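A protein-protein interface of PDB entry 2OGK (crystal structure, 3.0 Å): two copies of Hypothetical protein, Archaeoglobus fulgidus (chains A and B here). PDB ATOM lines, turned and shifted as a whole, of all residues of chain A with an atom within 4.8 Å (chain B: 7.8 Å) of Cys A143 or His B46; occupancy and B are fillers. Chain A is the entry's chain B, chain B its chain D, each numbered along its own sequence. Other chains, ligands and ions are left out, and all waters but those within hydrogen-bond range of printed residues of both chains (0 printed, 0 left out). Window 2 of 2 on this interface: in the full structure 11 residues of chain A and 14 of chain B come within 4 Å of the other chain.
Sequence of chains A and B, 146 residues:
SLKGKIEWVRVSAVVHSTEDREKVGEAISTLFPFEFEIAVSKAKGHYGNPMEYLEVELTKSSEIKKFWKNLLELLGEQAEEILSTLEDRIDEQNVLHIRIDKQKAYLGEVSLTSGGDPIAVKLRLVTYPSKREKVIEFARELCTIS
O of His B46 sits close to O of Cys A143 (3.5 Å).
The side-chain sulfur (SG) of Cys A143 is in hydrogen-bond range of the backbone carbonyl oxygen (O) of Arg A140, at 2.8 Å. The backbone NH (N) of Met B51 is in hydrogen-bond range of the backbone carbonyl oxygen (O) of Ala B43 (2.5 Å).
His B46 touches Glu A80 (CB to N, 3.8 Å). CD1 of Leu A83 touches O of Gly B45, at 3.8 Å. CA of His B46 touches CD1 of Leu A83 (3.5 Å). Arg A140 touches Ala B43. Arg A140 touches Tyr B53 (NH1 to OH, 3.9 Å).
Cys A143 touches just one residue of chain B: His B46. His B46 touches just these residues of chain A: Glu A80 (3.8 Å), Leu A83 (3.5 Å) and Cys A143 (3.5 Å). Printed residues of chain B within 4 Å of Arg A140: Ala B43 (3.4 Å) and Tyr B53 (3.9 Å). Of the printed residues of chain A, Gly B45 touches Leu A83.
Of the 10 printed residues of chain B, 4 touch a printed residue of chain A. Of the 9 printed residues of chain A, 4 touch a printed residue of chain B. Along chain A the printed residues that touch a printed residue of chain B span positions 80 to 143. Among the printed residues, no Asp or Glu carboxylate lies within 4 Å of a Lys or Arg side-chain nitrogen of the other chain.
No position is printed for both chains.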
ATOM      1  N   LEU A  72      29.703  10.655  14.102  1.00  0.00           N
ATOM      2  CA  LEU A  72      28.962  11.389  13.075  1.00  0.00           C
ATOM      3  C   LEU A  72      28.147  10.457  12.207  1.00  0.00           C
ATOM      4  O   LEU A  72      27.022  10.761  11.812  1.00  0.00           O
ATOM      5  CB  LEU A  72      29.924  12.125  12.160  1.00  0.00           C
ATOM      6  CG  LEU A  72      30.115  13.616  12.317  1.00  0.00           C
ATOM      7  CD1 LEU A  72      30.595  14.157  10.964  1.00  0.00           C
ATOM      8  CD2 LEU A  72      28.807  14.277  12.735  1.00  0.00           C
ATOM      9  N   ALA A  79      22.629  14.916  12.517  1.00  0.00           N
ATOM     10  CA  ALA A  79      23.642  15.965  12.564  1.00  0.00           C
ATOM     11  C   ALA A  79      23.111  17.304  12.060  1.00  0.00           C
ATOM     12  O   ALA A  79      23.720  18.344  12.275  1.00  0.00           O
ATOM     13  CB  ALA A  79      24.861  15.541  11.771  1.00  0.00           C
ATOM     14  N   GLU A  80      21.966  17.272  11.395  1.00  0.00           N
ATOM     15  CA  GLU A  80      21.360  18.496  10.891  1.00  0.00           C
ATOM     16  C   GLU A  80      20.846  19.312  12.082  1.00  0.00           C
ATOM     17  O   GLU A  80      20.859  20.544  12.063  1.00  0.00           O
ATOM     18  CB  GLU A  80      20.206  18.163   9.917  1.00  0.00           C
ATOM     19  N   LEU A  83      23.880  21.228  13.687  1.00  0.00           N
ATOM     20  CA  LEU A  83      24.245  22.420  12.915  1.00  0.00           C
ATOM     21  C   LEU A  83      23.273  23.597  13.043  1.00  0.00           C
ATOM     22  O   LEU A  83      23.681  24.756  13.019  1.00  0.00           O
ATOM     23  CB  LEU A  83      24.403  22.053  11.432  1.00  0.00           C
ATOM     24  CG  LEU A  83      25.587  21.155  11.053  1.00  0.00           C
ATOM     25  CD1 LEU A  83      25.514  20.754   9.592  1.00  0.00           C
ATOM     26  CD2 LEU A  83      26.874  21.897  11.331  1.00  0.00           C
ATOM     27  N   ALA A 139      33.221  24.308  13.322  1.00  0.00           N
ATOM     28  CA  ALA A 139      32.259  23.282  13.726  1.00  0.00           C
ATOM     29  C   ALA A 139      31.597  22.748  12.464  1.00  0.00           C
ATOM     30  O   ALA A 139      31.543  21.535  12.239  1.00  0.00           O
ATOM     31  CB  ALA A 139      31.206  23.882  14.657  1.00  0.00           C
ATOM     32  N   ARG A 140      31.093  23.673  11.651  1.00  0.00           N
ATOM     33  CA  ARG A 140      30.465  23.324  10.389  1.00  0.00           C
ATOM     34  C   ARG A 140      31.430  22.390   9.664  1.00  0.00           C
ATOM     35  O   ARG A 140      31.032  21.359   9.136  1.00  0.00           O
ATOM     36  CB  ARG A 140      30.257  24.577   9.540  1.00  0.00           C
ATOM     37  CG  ARG A 140      29.639  25.754  10.275  1.00  0.00           C
ATOM     38  CD  ARG A 140      28.145  25.889  10.007  1.00  0.00           C
ATOM     39  NE  ARG A 140      27.636  27.148  10.549  1.00  0.00           N
ATOM     40  CZ  ARG A 140      26.368  27.551  10.476  1.00  0.00           C
ATOM     41  NH1 ARG A 140      25.449  26.792   9.879  1.00  0.00           N
ATOM     42  NH2 ARG A 140      26.020  28.727  10.995  1.00  0.00           N
ATOM     43  N   GLU A 141      32.707  22.754   9.650  1.00  0.00           N
ATOM     44  CA  GLU A 141      33.709  21.938   8.980  1.00  0.00           C
ATOM     45  C   GLU A 141      33.609  20.452   9.333  1.00  0.00           C
ATOM     46  O   GLU A 141      33.814  19.592   8.472  1.00  0.00           O
ATOM     47  CB  GLU A 141      35.115  22.457   9.293  1.00  0.00           C
ATOM     48  CG  GLU A 141      36.229  21.618   8.666  1.00  0.00           C
ATOM     49  CD  GLU A 141      37.273  22.466   7.970  1.00  0.00           C
ATOM     50  OE1 GLU A 141      36.906  23.229   7.050  1.00  0.00           O
ATOM     51  OE2 GLU A 141      38.462  22.373   8.339  1.00  0.00           O
ATOM     52  N   LEU A 142      33.296  20.147  10.591  1.00  0.00           N
ATOM     53  CA  LEU A 142      33.168  18.757  11.017  1.00  0.00           C
ATOM     54  C   LEU A 142      31.812  18.188  10.610  1.00  0.00           C
ATOM     55  O   LEU A 142      31.061  17.695  11.446  1.00  0.00           O
ATOM     56  CB  LEU A 142      33.363  18.652  12.531  1.00  0.00           C
ATOM     57  CG  LEU A 142      34.782  18.969  13.037  1.00  0.00           C
ATOM     58  CD1 LEU A 142      34.799  19.121  14.547  1.00  0.00           C
ATOM     59  CD2 LEU A 142      35.719  17.856  12.620  1.00  0.00           C
ATOM     60  N   CYS A 143      31.522  18.282   9.307  1.00  0.00           N
ATOM     61  CA  CYS A 143      30.280  17.792   8.691  1.00  0.00           C
ATOM     62  C   CYS A 143      30.578  17.345   7.245  1.00  0.00           C
ATOM     63  O   CYS A 143      29.888  17.822   6.316  1.00  0.00           O
ATOM     64  CB  CYS A 143      29.202  18.895   8.670  1.00  0.00           C
ATOM     65  SG  CYS A 143      29.360  20.137   7.321  1.00  0.00           S
ATOM     66  N   ALA B  43      22.735  28.547   5.155  1.00  0.00           N
ATOM     67  CA  ALA B  43      23.995  27.846   5.361  1.00  0.00           C
ATOM     68  C   ALA B  43      23.920  26.464   4.735  1.00  0.00           C
ATOM     69  O   ALA B  43      22.873  26.075   4.228  1.00  0.00           O
ATOM     70  CB  ALA B  43      24.298  27.734   6.849  1.00  0.00           C
ATOM     71  N   LYS B  44      25.033  25.734   4.771  1.00  0.00           N
ATOM     72  CA  LYS B  44      25.100  24.389   4.206  1.00  0.00           C
ATOM     73  C   LYS B  44      24.635  23.327   5.212  1.00  0.00           C
ATOM     74  O   LYS B  44      25.157  23.228   6.327  1.00  0.00           O
ATOM     75  CB  LYS B  44      26.521  24.090   3.740  1.00  0.00           C
ATOM     76  N   GLY B  45      23.651  22.534   4.792  1.00  0.00           N
ATOM     77  CA  GLY B  45      23.086  21.498   5.634  1.00  0.00           C
ATOM     78  C   GLY B  45      24.042  20.426   6.108  1.00  0.00           C
ATOM     79  O   GLY B  45      25.240  20.476   5.817  1.00  0.00           O
ATOM     80  N   HIS B  46      23.492  19.462   6.854  1.00  0.00           N
ATOM     81  CA  HIS B  46      24.257  18.338   7.399  1.00  0.00           C
ATOM     82  C   HIS B  46      25.228  17.849   6.334  1.00  0.00           C
ATOM     83  O   HIS B  46      26.434  17.784   6.557  1.00  0.00           O
ATOM     84  CB  HIS B  46      23.313  17.208   7.823  1.00  0.00           C
ATOM     85  N   TYR B  47      24.686  17.505   5.172  1.00  0.00           N
ATOM     86  CA  TYR B  47      25.508  17.059   4.059  1.00  0.00           C
ATOM     87  C   TYR B  47      26.111  18.344   3.498  1.00  0.00           C
ATOM     88  O   TYR B  47      26.591  19.186   4.265  1.00  0.00           O
ATOM     89  CB  TYR B  47      24.649  16.363   3.004  1.00  0.00           C
ATOM     90  N   GLY B  48      26.077  18.508   2.177  1.00  0.00           N
ATOM     91  CA  GLY B  48      26.621  19.715   1.583  1.00  0.00           C
ATOM     92  C   GLY B  48      25.523  20.621   1.059  1.00  0.00           C
ATOM     93  O   GLY B  48      25.774  21.736   0.603  1.00  0.00           O
ATOM     94  N   ASN B  49      24.289  20.139   1.142  1.00  0.00           N
ATOM     95  CA  ASN B  49      23.132  20.881   0.654  1.00  0.00           C
ATOM     96  C   ASN B  49      22.819  22.210   1.308  1.00  0.00           C
ATOM     97  O   ASN B  49      22.754  22.318   2.529  1.00  0.00           O
ATOM     98  CB  ASN B  49      21.873  20.026   0.738  1.00  0.00           C
ATOM     99  CG  ASN B  49      21.817  18.987  -0.335  1.00  0.00           C
ATOM    100  OD1 ASN B  49      22.122  17.817  -0.104  1.00  0.00           O
ATOM    101  ND2 ASN B  49      21.437  19.410  -1.533  1.00  0.00           N
ATOM    102  N   PRO B  50      22.604  23.243   0.482  1.00  0.00           N
ATOM    103  CA  PRO B  50      22.277  24.598   0.932  1.00  0.00           C
ATOM    104  C   PRO B  50      20.963  24.587   1.712  1.00  0.00           C
ATOM    105  O   PRO B  50      19.922  24.154   1.211  1.00  0.00           O
ATOM    106  CB  PRO B  50      22.167  25.373  -0.376  1.00  0.00           C
ATOM    107  CG  PRO B  50      23.200  24.715  -1.222  1.00  0.00           C
ATOM    108  CD  PRO B  50      22.947  23.245  -0.953  1.00  0.00           C
ATOM    109  N   MET B  51      21.031  25.075   2.946  1.00  0.00           N
ATOM    110  CA  MET B  51      19.887  25.128   3.844  1.00  0.00           C
ATOM    111  C   MET B  51      19.397  26.553   4.076  1.00  0.00           C
ATOM    112  O   MET B  51      20.136  27.524   3.868  1.00  0.00           O
ATOM    113  CB  MET B  51      20.263  24.521   5.202  1.00  0.00           C
ATOM    114  CG  MET B  51      20.450  23.027   5.201  1.00  0.00           C
ATOM    115  SD  MET B  51      18.884  22.176   5.051  1.00  0.00           S
ATOM    116  CE  MET B  51      18.873  21.705   3.292  1.00  0.00           C
ATOM    117  N   TYR B  53      17.253  28.639   7.169  1.00  0.00           N
ATOM    118  CA  TYR B  53      16.807  28.551   8.564  1.00  0.00           C
ATOM    119  C   TYR B  53      15.790  29.635   8.895  1.00  0.00           C
ATOM    120  O   TYR B  53      15.968  30.794   8.535  1.00  0.00           O
ATOM    121  CB  TYR B  53      17.993  28.686   9.515  1.00  0.00           C
ATOM    122  CG  TYR B  53      19.098  27.675   9.300  1.00  0.00           C
ATOM    123  CD1 TYR B  53      18.829  26.306   9.266  1.00  0.00           C
ATOM    124  CD2 TYR B  53      20.426  28.086   9.199  1.00  0.00           C
ATOM    125  CE1 TYR B  53      19.862  25.367   9.146  1.00  0.00           C
ATOM    126  CE2 TYR B  53      21.464  27.158   9.081  1.00  0.00           C
ATOM    127  CZ  TYR B  53      21.179  25.800   9.057  1.00  0.00           C
ATOM    128  OH  TYR B  53      22.214  24.889   8.972  1.00  0.00           O
